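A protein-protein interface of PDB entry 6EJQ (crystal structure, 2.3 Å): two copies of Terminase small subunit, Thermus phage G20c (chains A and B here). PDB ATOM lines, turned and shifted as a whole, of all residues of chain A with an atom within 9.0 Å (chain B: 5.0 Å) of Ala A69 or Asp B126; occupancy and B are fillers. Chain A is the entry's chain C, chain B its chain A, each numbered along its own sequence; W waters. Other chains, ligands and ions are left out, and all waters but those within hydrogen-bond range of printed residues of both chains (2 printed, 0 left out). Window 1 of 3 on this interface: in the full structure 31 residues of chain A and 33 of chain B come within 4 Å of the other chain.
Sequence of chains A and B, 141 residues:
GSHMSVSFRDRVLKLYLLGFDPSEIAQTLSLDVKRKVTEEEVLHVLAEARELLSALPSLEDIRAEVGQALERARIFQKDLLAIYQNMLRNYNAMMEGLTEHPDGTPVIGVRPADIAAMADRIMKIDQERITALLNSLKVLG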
ATOM      1  N   ASP A  61      25.322  32.636 -26.031  1.00  0.00           N
ATOM      2  CA  ASP A  61      24.283  32.627 -27.064  1.00  0.00           C
ATOM      3  C   ASP A  61      23.432  31.355 -26.971  1.00  0.00           C
ATOM      4  O   ASP A  61      22.212  31.414 -27.102  1.00  0.00           O
ATOM      5  CB  ASP A  61      24.884  32.770 -28.473  1.00  0.00           C
ATOM      6  CG  ASP A  61      25.624  34.112 -28.688  1.00  0.00           C
ATOM      7  OD1 ASP A  61      25.764  34.920 -27.729  1.00  0.00           O
ATOM      8  OD2 ASP A  61      26.087  34.350 -29.831  1.00  0.00           O
ATOM      9  N   ILE A  62      24.078  30.219 -26.717  1.00  0.00           N
ATOM     10  CA  ILE A  62      23.377  28.949 -26.546  1.00  0.00           C
ATOM     11  C   ILE A  62      22.412  28.999 -25.358  1.00  0.00           C
ATOM     12  O   ILE A  62      21.312  28.476 -25.451  1.00  0.00           O
ATOM     13  CB  ILE A  62      24.360  27.754 -26.429  1.00  0.00           C
ATOM     14  CG1 ILE A  62      25.092  27.554 -27.759  1.00  0.00           C
ATOM     15  CG2 ILE A  62      23.633  26.461 -26.047  1.00  0.00           C
ATOM     16  CD1 ILE A  62      26.331  26.697 -27.655  1.00  0.00           C
ATOM     17  N   ARG A  63      22.811  29.628 -24.257  1.00  0.00           N
ATOM     18  CA  ARG A  63      21.897  29.835 -23.119  1.00  0.00           C
ATOM     19  C   ARG A  63      20.671  30.683 -23.492  1.00  0.00           C
ATOM     20  O   ARG A  63      19.553  30.403 -23.043  1.00  0.00           O
ATOM     21  CB  ARG A  63      22.620  30.469 -21.932  1.00  0.00           C
ATOM     22  CG  ARG A  63      23.531  29.510 -21.189  1.00  0.00           C
ATOM     23  CD  ARG A  63      23.969  30.071 -19.839  1.00  0.00           C
ATOM     24  NE  ARG A  63      24.889  31.201 -19.977  1.00  0.00           N
ATOM     25  CZ  ARG A  63      26.190  31.116 -20.287  1.00  0.00           C
ATOM     26  NH1 ARG A  63      26.784  29.941 -20.509  1.00  0.00           N
ATOM     27  NH2 ARG A  63      26.913  32.232 -20.384  1.00  0.00           N
ATOM     28  N   ALA A  64      20.891  31.705 -24.317  1.00  0.00           N
ATOM     29  CA  ALA A  64      19.795  32.510 -24.862  1.00  0.00           C
ATOM     30  C   ALA A  64      18.835  31.634 -25.680  1.00  0.00           C
ATOM     31  O   ALA A  64      17.630  31.781 -25.547  1.00  0.00           O
ATOM     32  CB  ALA A  64      20.316  33.678 -25.705  1.00  0.00           C
ATOM     33  N   GLU A  65      19.370  30.722 -26.499  1.00  0.00           N
ATOM     34  CA  GLU A  65      18.528  29.772 -27.257  1.00  0.00           C
ATOM     35  C   GLU A  65      17.735  28.867 -26.332  1.00  0.00           C
ATOM     36  O   GLU A  65      16.571  28.584 -26.601  1.00  0.00           O
ATOM     37  CB  GLU A  65      19.346  28.910 -28.209  1.00  0.00           C
ATOM     38  CG  GLU A  65      19.955  29.683 -29.363  1.00  0.00           C
ATOM     39  CD  GLU A  65      18.954  30.098 -30.416  1.00  0.00           C
ATOM     40  OE1 GLU A  65      17.801  29.609 -30.403  1.00  0.00           O
ATOM     41  OE2 GLU A  65      19.342  30.915 -31.276  1.00  0.00           O
ATOM     42  N   VAL A  66      18.360  28.436 -25.241  1.00  0.00           N
ATOM     43  CA  VAL A  66      17.681  27.617 -24.241  1.00  0.00           C
ATOM     44  C   VAL A  66      16.553  28.419 -23.585  1.00  0.00           C
ATOM     45  O   VAL A  66      15.456  27.897 -23.392  1.00  0.00           O
ATOM     46  CB  VAL A  66      18.667  27.058 -23.184  1.00  0.00           C
ATOM     47  CG1 VAL A  66      17.935  26.403 -22.012  1.00  0.00           C
ATOM     48  CG2 VAL A  66      19.607  26.047 -23.827  1.00  0.00           C
ATOM     49  N   GLY A  67      16.815  29.684 -23.260  1.00  0.00           N
ATOM     50  CA  GLY A  67      15.780  30.545 -22.702  1.00  0.00           C
ATOM     51  C   GLY A  67      14.592  30.754 -23.629  1.00  0.00           C
ATOM     52  O   GLY A  67      13.440  30.647 -23.196  1.00  0.00           O
ATOM     53  N   GLN A  68      14.871  31.049 -24.897  1.00  0.00           N
ATOM     54  CA  GLN A  68      13.827  31.225 -25.914  1.00  0.00           C
ATOM     55  C   GLN A  68      13.004  29.953 -26.115  1.00  0.00           C
ATOM     56  O   GLN A  68      11.776  30.018 -26.195  1.00  0.00           O
ATOM     57  CB  GLN A  68      14.424  31.653 -27.253  1.00  0.00           C
ATOM     58  CG  GLN A  68      14.993  33.061 -27.274  1.00  0.00           C
ATOM     59  CD  GLN A  68      15.536  33.451 -28.638  1.00  0.00           C
ATOM     60  OE1 GLN A  68      14.792  33.920 -29.490  1.00  0.00           O
ATOM     61  NE2 GLN A  68      16.843  33.257 -28.851  1.00  0.00           N
ATOM     62  N   ALA A  69      13.689  28.809 -26.204  1.00  0.00           N
ATOM     63  CA  ALA A  69      13.047  27.499 -26.364  1.00  0.00           C
ATOM     64  C   ALA A  69      12.082  27.186 -25.224  1.00  0.00           C
ATOM     65  O   ALA A  69      10.987  26.676 -25.464  1.00  0.00           O
ATOM     66  CB  ALA A  69      14.090  26.398 -26.478  1.00  0.00           C
ATOM     67  N   LEU A  70      12.485  27.492 -23.994  1.00  0.00           N
ATOM     68  CA  LEU A  70      11.620  27.294 -22.835  1.00  0.00           C
ATOM     69  C   LEU A  70      10.412  28.233 -22.839  1.00  0.00           C
ATOM     70  O   LEU A  70       9.313  27.832 -22.444  1.00  0.00           O
ATOM     71  CB  LEU A  70      12.407  27.434 -21.531  1.00  0.00           C
ATOM     72  CG  LEU A  70      13.528  26.401 -21.290  1.00  0.00           C
ATOM     73  CD1 LEU A  70      14.060  26.501 -19.871  1.00  0.00           C
ATOM     74  CD2 LEU A  70      13.090  24.974 -21.614  1.00  0.00           C
ATOM     75  N   GLU A  71      10.610  29.470 -23.292  1.00  0.00           N
ATOM     76  CA  GLU A  71       9.518  30.429 -23.400  1.00  0.00           C
ATOM     77  C   GLU A  71       8.528  29.984 -24.479  1.00  0.00           C
ATOM     78  O   GLU A  71       7.319  30.002 -24.253  1.00  0.00           O
ATOM     79  CB  GLU A  71      10.061  31.826 -23.691  1.00  0.00           C
ATOM     80  CG  GLU A  71       9.026  32.948 -23.688  1.00  0.00           C
ATOM     81  CD  GLU A  71       8.222  33.038 -22.400  1.00  0.00           C
ATOM     82  OE1 GLU A  71       8.791  32.816 -21.311  1.00  0.00           O
ATOM     83  OE2 GLU A  71       7.014  33.335 -22.490  1.00  0.00           O
ATOM     84  N   ARG A  72       9.041  29.559 -25.630  1.00  0.00           N
ATOM     85  CA  ARG A  72       8.197  29.031 -26.700  1.00  0.00           C
ATOM     86  C   ARG A  72       7.403  27.821 -26.212  1.00  0.00           C
ATOM     87  O   ARG A  72       6.200  27.702 -26.474  1.00  0.00           O
ATOM     88  CB  ARG A  72       9.025  28.643 -27.928  1.00  0.00           C
ATOM     89  CG  ARG A  72       8.196  28.545 -29.197  1.00  0.00           C
ATOM     90  CD  ARG A  72       8.802  27.602 -30.225  1.00  0.00           C
ATOM     91  NE  ARG A  72      10.151  27.988 -30.631  1.00  0.00           N
ATOM     92  CZ  ARG A  72      10.457  28.961 -31.494  1.00  0.00           C
ATOM     93  NH1 ARG A  72       9.517  29.716 -32.059  1.00  0.00           N
ATOM     94  NH2 ARG A  72      11.731  29.192 -31.791  1.00  0.00           N
ATOM     95  N   ALA A  73       8.076  26.941 -25.478  1.00  0.00           N
ATOM     96  CA  ALA A  73       7.433  25.763 -24.921  1.00  0.00           C
ATOM     97  C   ALA A  73       6.316  26.141 -23.957  1.00  0.00           C
ATOM     98  O   ALA A  73       5.315  25.438 -23.901  1.00  0.00           O
ATOM     99  CB  ALA A  73       8.453  24.846 -24.245  1.00  0.00           C
ATOM    100  N   ARG A  74       6.483  27.234 -23.209  1.00  0.00           N
ATOM    101  CA  ARG A  74       5.406  27.750 -22.333  1.00  0.00           C
ATOM    102  C   ARG A  74       4.153  28.184 -23.104  1.00  0.00           C
ATOM    103  O   ARG A  74       3.033  27.945 -22.655  1.00  0.00           O
ATOM    104  CB  ARG A  74       5.886  28.923 -21.469  1.00  0.00           C
ATOM    105  CG  ARG A  74       6.748  28.511 -20.293  1.00  0.00           C
ATOM    106  CD  ARG A  74       6.855  29.613 -19.255  1.00  0.00           C
ATOM    107  NE  ARG A  74       7.385  29.092 -17.993  1.00  0.00           N
ATOM    108  CZ  ARG A  74       8.673  28.871 -17.727  1.00  0.00           C
ATOM    109  NH1 ARG A  74       9.630  29.117 -18.631  1.00  0.00           N
ATOM    110  NH2 ARG A  74       9.008  28.394 -16.532  1.00  0.00           N
ATOM    111  N   ILE A  75       4.364  28.807 -24.262  1.00  0.00           N
ATOM    112  CA  ILE A  75       3.282  29.244 -25.134  1.00  0.00           C
ATOM    113  C   ILE A  75       2.467  28.026 -25.579  1.00  0.00           C
ATOM    114  O   ILE A  75       1.249  27.981 -25.395  1.00  0.00           O
ATOM    115  CB  ILE A  75       3.839  30.027 -26.349  1.00  0.00           C
ATOM    116  CG1 ILE A  75       4.483  31.342 -25.886  1.00  0.00           C
ATOM    117  CG2 ILE A  75       2.756  30.323 -27.380  1.00  0.00           C
ATOM    118  CD1 ILE A  75       5.428  31.942 -26.909  1.00  0.00           C
ATOM    119  N   PHE A  76       3.145  27.028 -26.135  1.00  0.00           N
ATOM    120  CA  PHE A  76       2.487  25.775 -26.507  1.00  0.00           C
ATOM    121  C   PHE A  76       1.790  25.107 -25.323  1.00  0.00           C
ATOM    122  O   PHE A  76       0.672  24.612 -25.464  1.00  0.00           O
ATOM    123  CB  PHE A  76       3.480  24.782 -27.120  1.00  0.00           C
ATOM    124  CG  PHE A  76       4.048  25.199 -28.461  1.00  0.00           C
ATOM    125  CD1 PHE A  76       3.247  25.739 -29.454  1.00  0.00           C
ATOM    126  CD2 PHE A  76       5.385  24.980 -28.749  1.00  0.00           C
ATOM    127  CE1 PHE A  76       3.776  26.093 -30.688  1.00  0.00           C
ATOM    128  CE2 PHE A  76       5.920  25.314 -29.983  1.00  0.00           C
ATOM    129  CZ  PHE A  76       5.116  25.880 -30.956  1.00  0.00           C
ATOM    130  N   GLN A  77       2.439  25.096 -24.165  1.00  0.00           N
ATOM    131  CA  GLN A  77       1.888  24.422 -22.982  1.00  0.00           C
ATOM    132  C   GLN A  77       0.571  25.067 -22.565  1.00  0.00           C
ATOM    133  O   GLN A  77      -0.363  24.381 -22.166  1.00  0.00           O
ATOM    134  CB  GLN A  77       2.888  24.441 -21.818  1.00  0.00           C
ATOM    135  CG  GLN A  77       2.541  23.496 -20.674  1.00  0.00           C
ATOM    136  CD  GLN A  77       3.538  23.550 -19.533  1.00  0.00           C
ATOM    137  OE1 GLN A  77       3.978  24.623 -19.132  1.00  0.00           O
ATOM    138  NE2 GLN A  77       3.887  22.388 -18.992  1.00  0.00           N
ATOM    139  N   ILE A 125       6.464  18.730 -21.044  1.00  0.00           N
ATOM    140  CA  ILE A 125       6.985  20.096 -21.209  1.00  0.00           C
ATOM    141  C   ILE A 125       7.579  20.613 -19.888  1.00  0.00           C
ATOM    142  O   ILE A 125       8.616  21.280 -19.901  1.00  0.00           O
ATOM    143  CB  ILE A 125       5.925  21.077 -21.784  1.00  0.00           C
ATOM    144  CG1 ILE A 125       5.580  20.691 -23.232  1.00  0.00           C
ATOM    145  CG2 ILE A 125       6.436  22.512 -21.760  1.00  0.00           C
ATOM    146  CD1 ILE A 125       4.329  21.341 -23.789  1.00  0.00           C
ATOM    147  N   GLU A 128      10.956  18.492 -19.534  1.00  0.00           N
ATOM    148  CA  GLU A 128      11.979  18.952 -20.501  1.00  0.00           C
ATOM    149  C   GLU A 128      12.536  20.339 -20.151  1.00  0.00           C
ATOM    150  O   GLU A 128      13.686  20.644 -20.482  1.00  0.00           O
ATOM    151  CB  GLU A 128      11.449  18.956 -21.947  1.00  0.00           C
ATOM    152  CG  GLU A 128      11.357  17.570 -22.577  1.00  0.00           C
ATOM    153  CD  GLU A 128      10.526  17.507 -23.863  1.00  0.00           C
ATOM    154  OE1 GLU A 128       9.565  18.301 -24.044  1.00  0.00           O
ATOM    155  OE2 GLU A 128      10.822  16.624 -24.697  1.00  0.00           O
ATOM    156  N   ARG A 129      11.719  21.168 -19.495  1.00  0.00           N
ATOM    157  CA  ARG A 129      12.158  22.468 -18.995  1.00  0.00           C
ATOM    158  C   ARG A 129      13.354  22.295 -18.069  1.00  0.00           C
ATOM    159  O   ARG A 129      14.406  22.915 -18.260  1.00  0.00           O
ATOM    160  CB  ARG A 129      11.008  23.181 -18.259  1.00  0.00           C
ATOM    161  CG  ARG A 129      11.396  24.479 -17.571  1.00  0.00           C
ATOM    162  CD  ARG A 129      10.295  25.523 -17.605  1.00  0.00           C
ATOM    163  NE  ARG A 129       9.088  25.113 -16.883  1.00  0.00           N
ATOM    164  CZ  ARG A 129       7.877  24.887 -17.412  1.00  0.00           C
ATOM    165  NH1 ARG A 129       7.623  25.011 -18.724  1.00  0.00           N
ATOM    166  NH2 ARG A 129       6.892  24.519 -16.601  1.00  0.00           N
ATOM    167  N   ALA A 132      16.721  20.792 -19.611  1.00  0.00           N
ATOM    168  CA  ALA A 132      17.456  21.815 -20.377  1.00  0.00           C
ATOM    169  C   ALA A 132      18.154  22.825 -19.452  1.00  0.00           C
ATOM    170  O   ALA A 132      19.301  23.214 -19.722  1.00  0.00           O
ATOM    171  CB  ALA A 132      16.537  22.536 -21.360  1.00  0.00           C
ATOM    172  N   GLN B  77      10.834  25.659 -39.421  1.00  0.00           N
ATOM    173  CA  GLN B  77      10.208  25.998 -38.148  1.00  0.00           C
ATOM    174  C   GLN B  77       9.194  27.150 -38.283  1.00  0.00           C
ATOM    175  O   GLN B  77       8.128  27.118 -37.668  1.00  0.00           O
ATOM    176  CB  GLN B  77      11.277  26.349 -37.109  1.00  0.00           C
ATOM    177  CG  GLN B  77      10.760  26.490 -35.688  1.00  0.00           C
ATOM    178  CD  GLN B  77      11.886  26.661 -34.694  1.00  0.00           C
ATOM    179  OE1 GLN B  77      12.776  27.505 -34.873  1.00  0.00           O
ATOM    180  NE2 GLN B  77      11.851  25.866 -33.628  1.00  0.00           N
ATOM    181  N   ILE B 122       7.927  21.394 -33.486  1.00  0.00           N
ATOM    182  CA  ILE B 122       8.483  22.744 -33.440  1.00  0.00           C
ATOM    183  C   ILE B 122       9.483  22.879 -32.282  1.00  0.00           C
ATOM    184  O   ILE B 122      10.565  23.446 -32.460  1.00  0.00           O
ATOM    185  CB  ILE B 122       7.365  23.804 -33.341  1.00  0.00           C
ATOM    186  CG1 ILE B 122       6.540  23.814 -34.637  1.00  0.00           C
ATOM    187  CG2 ILE B 122       7.938  25.188 -33.073  1.00  0.00           C
ATOM    188  CD1 ILE B 122       5.134  24.349 -34.456  1.00  0.00           C
ATOM    189  N   MET B 123       9.111  22.366 -31.111  1.00  0.00           N
ATOM    190  CA  MET B 123      10.002  22.373 -29.951  1.00  0.00           C
ATOM    191  C   MET B 123      11.276  21.557 -30.170  1.00  0.00           C
ATOM    192  O   MET B 123      12.338  21.948 -29.695  1.00  0.00           O
ATOM    193  CB  MET B 123       9.271  21.892 -28.699  1.00  0.00           C
ATOM    194  CG  MET B 123       8.222  22.876 -28.232  1.00  0.00           C
ATOM    195  SD  MET B 123       7.422  22.419 -26.693  1.00  0.00           S
ATOM    196  CE  MET B 123       6.476  20.998 -27.228  1.00  0.00           C
ATOM    197  N   LYS B 124      11.167  20.447 -30.896  1.00  0.00           N
ATOM    198  CA  LYS B 124      12.328  19.621 -31.238  1.00  0.00           C
ATOM    199  C   LYS B 124      13.344  20.390 -32.064  1.00  0.00           C
ATOM    200  O   LYS B 124      14.545  20.193 -31.893  1.00  0.00           O
ATOM    201  CB  LYS B 124      11.919  18.352 -32.006  1.00  0.00           C
ATOM    202  CG  LYS B 124      11.278  17.282 -31.143  1.00  0.00           C
ATOM    203  CD  LYS B 124      12.307  16.319 -30.571  1.00  0.00           C
ATOM    204  CE  LYS B 124      11.702  15.409 -29.500  1.00  0.00           C
ATOM    205  NZ  LYS B 124      10.728  14.427 -30.053  1.00  0.00           N
ATOM    206  N   ILE B 125      12.871  21.250 -32.962  1.00  0.00           N
ATOM    207  CA  ILE B 125      13.780  22.049 -33.793  1.00  0.00           C
ATOM    208  C   ILE B 125      14.672  22.946 -32.931  1.00  0.00           C
ATOM    209  O   ILE B 125      15.859  23.103 -33.232  1.00  0.00           O
ATOM    210  CB  ILE B 125      13.033  22.833 -34.901  1.00  0.00           C
ATOM    211  CG1 ILE B 125      12.495  21.851 -35.953  1.00  0.00           C
ATOM    212  CG2 ILE B 125      13.946  23.854 -35.583  1.00  0.00           C
ATOM    213  CD1 ILE B 125      11.498  22.452 -36.921  1.00  0.00           C
ATOM    214  N   ASP B 126      14.117  23.504 -31.857  1.00  0.00           N
ATOM    215  CA  ASP B 126      14.913  24.289 -30.910  1.00  0.00           C
ATOM    216  C   ASP B 126      15.940  23.394 -30.212  1.00  0.00           C
ATOM    217  O   ASP B 126      17.110  23.770 -30.094  1.00  0.00           O
ATOM    218  CB  ASP B 126      14.054  24.955 -29.831  1.00  0.00           C
ATOM    219  CG  ASP B 126      13.105  26.024 -30.365  1.00  0.00           C
ATOM    220  OD1 ASP B 126      13.397  26.703 -31.364  1.00  0.00           O
ATOM    221  OD2 ASP B 126      12.049  26.207 -29.723  1.00  0.00           O
ATOM    222  N   GLN B 127      15.473  22.223 -29.756  1.00  0.00           N
ATOM    223  CA  GLN B 127      16.298  21.230 -29.065  1.00  0.00           C
ATOM    224  C   GLN B 127      17.482  20.819 -29.940  1.00  0.00           C
ATOM    225  O   GLN B 127      18.632  20.850 -29.502  1.00  0.00           O
ATOM    226  CB  GLN B 127      15.460  19.994 -28.672  1.00  0.00           C
ATOM    227  CG  GLN B 127      14.404  20.241 -27.592  1.00  0.00           C
ATOM    228  CD  GLN B 127      13.374  19.117 -27.475  1.00  0.00           C
ATOM    229  OE1 GLN B 127      13.685  17.945 -27.708  1.00  0.00           O
ATOM    230  NE2 GLN B 127      12.146  19.470 -27.091  1.00  0.00           N
ATOM    231  N   GLU B 128      17.181  20.475 -31.185  1.00  0.00           N
ATOM    232  CA  GLU B 128      18.189  20.104 -32.179  1.00  0.00           C
ATOM    233  C   GLU B 128      19.190  21.229 -32.471  1.00  0.00           C
ATOM    234  O   GLU B 128      20.364  20.958 -32.722  1.00  0.00           O
ATOM    235  CB  GLU B 128      17.526  19.624 -33.473  1.00  0.00           C
ATOM    236  CG  GLU B 128      17.069  18.175 -33.394  1.00  0.00           C
ATOM    237  CD  GLU B 128      15.944  17.785 -34.358  1.00  0.00           C
ATOM    238  OE1 GLU B 128      15.619  18.543 -35.311  1.00  0.00           O
ATOM    239  OE2 GLU B 128      15.377  16.685 -34.145  1.00  0.00           O
ATOM    240  N   ARG B 129      18.728  22.477 -32.436  1.00  0.00           N
ATOM    241  CA  ARG B 129      19.605  23.636 -32.602  1.00  0.00           C
ATOM    242  C   ARG B 129      20.591  23.741 -31.447  1.00  0.00           C
ATOM    243  O   ARG B 129      21.790  23.886 -31.658  1.00  0.00           O
ATOM    244  CB  ARG B 129      18.784  24.935 -32.729  1.00  0.00           C
ATOM    245  CG  ARG B 129      19.618  26.201 -32.815  1.00  0.00           C
ATOM    246  CD  ARG B 129      18.890  27.328 -33.540  1.00  0.00           C
ATOM    247  NE  ARG B 129      17.735  27.718 -32.760  1.00  0.00           N
ATOM    248  CZ  ARG B 129      16.454  27.555 -33.089  1.00  0.00           C
ATOM    249  NH1 ARG B 129      16.058  27.039 -34.256  1.00  0.00           N
ATOM    250  NH2 ARG B 129      15.546  27.940 -32.205  1.00  0.00           N
ATOM    251  N   ILE B 130      20.065  23.674 -30.236  1.00  0.00           N
ATOM    252  CA  ILE B 130      20.875  23.737 -29.023  1.00  0.00           C
ATOM    253  C   ILE B 130      21.923  22.599 -28.981  1.00  0.00           C
ATOM    254  O   ILE B 130      23.097  22.837 -28.687  1.00  0.00           O
ATOM    255  CB  ILE B 130      19.946  23.727 -27.783  1.00  0.00           C
ATOM    256  CG1 ILE B 130      19.212  25.081 -27.691  1.00  0.00           C
ATOM    257  CG2 ILE B 130      20.706  23.442 -26.492  1.00  0.00           C
ATOM    258  CD1 ILE B 130      17.878  25.034 -26.973  1.00  0.00           C
HETATM  259  O   HOH W   1       9.518  21.295 -24.238  1.00  0.00           O
HETATM  260  O   HOH W   2      10.870  24.985 -27.633  1.00  0.00           O
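The guanidinium group of Arg A72 is in salt-bridge range of the side-chain carboxylate of Asp B126 (2.8 Å).
The guanidinium group (NE) of Arg B129 is in salt-bridge range of the side-chain carboxylate (OE1) of Glu A65, 3.0 Å away.
Water W2 bridges the side-chain carboxylate (OD2) of Asp B126 (2.7 Å) and the backbone carbonyl oxygen (O) of Ala A69 (2.8 Å).
Water W1 bridges the side-chain carboxylate (OE1) of Glu A128 and the side-chain sulfur (SD) of Met B123.
Among the printed residues, Asp or Glu carboxylates within 4 Å of a Lys or Arg side-chain nitrogen of the other chain: Glu A65 with Arg B129 (3.0 Å) and Arg A72 with Asp B126 (2.8 Å).
4 positions are printed for both chains.
Of the 11 pairs that touch across the chains among the printed residues, none has its exchanged pair printed and touching as well.
OD1 of Asp B126 is in salt-bridge range of NH2 of Arg B129 (2.6 Å).
O of Ile B122 is in hydrogen-bond range of NE2 of Gln B77.
OD1 of Asp B126 is in hydrogen-bond range of NE2 of Gln B77, 2.9 Å away.
The guanidinium group (NH1) of Arg B129 lies within hydrogen-bond range of the side-chain amide oxygen (OE1) of Gln B77 (3.4 Å).
CD1 of Ile B130 touches O of Glu A65, 3.8 Å away.
Val A66 touches Ile B130 (CG2 to CD1, 3.7 Å).
Ala A69 touches Asp B126.
Gln B77 touches Arg A72.
CG2 of Ile B122 touches CD of Arg A72, 3.8 Å away.
CB of Ala A73 touches SD of Met B123, 3.6 Å away.
Phe A76 touches Ile B122.
CD2 of Phe A76 touches CG of Met B123, at 3.6 Å.
OE2 of Glu A128 touches NE2 of Gln B127, at 3.9 Å.
Ala A69 touches one residue of chain B.
Printed residues of chain A within 4 Å of Asp B126: Ala A69 (3.7 Å) and Arg A72 (2.8 Å).
Printed residues of chain B within 4 Å of Phe A76: Ile B122 and Met B123.
Of the printed residues of chain B, Ala A73 touches Met B123.
Printed residues of chain A within 4 Å of Met B123: Ala A73 and Phe A76.
Of the printed residues of chain B, Arg A72 touches Gln B77 (3.7 Å), Ile B122 (3.8 Å) and Asp B126 (2.8 Å).
The nearest printed residue of chain A that does not touch Ile B122 is Ala A69 (7.5 Å).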
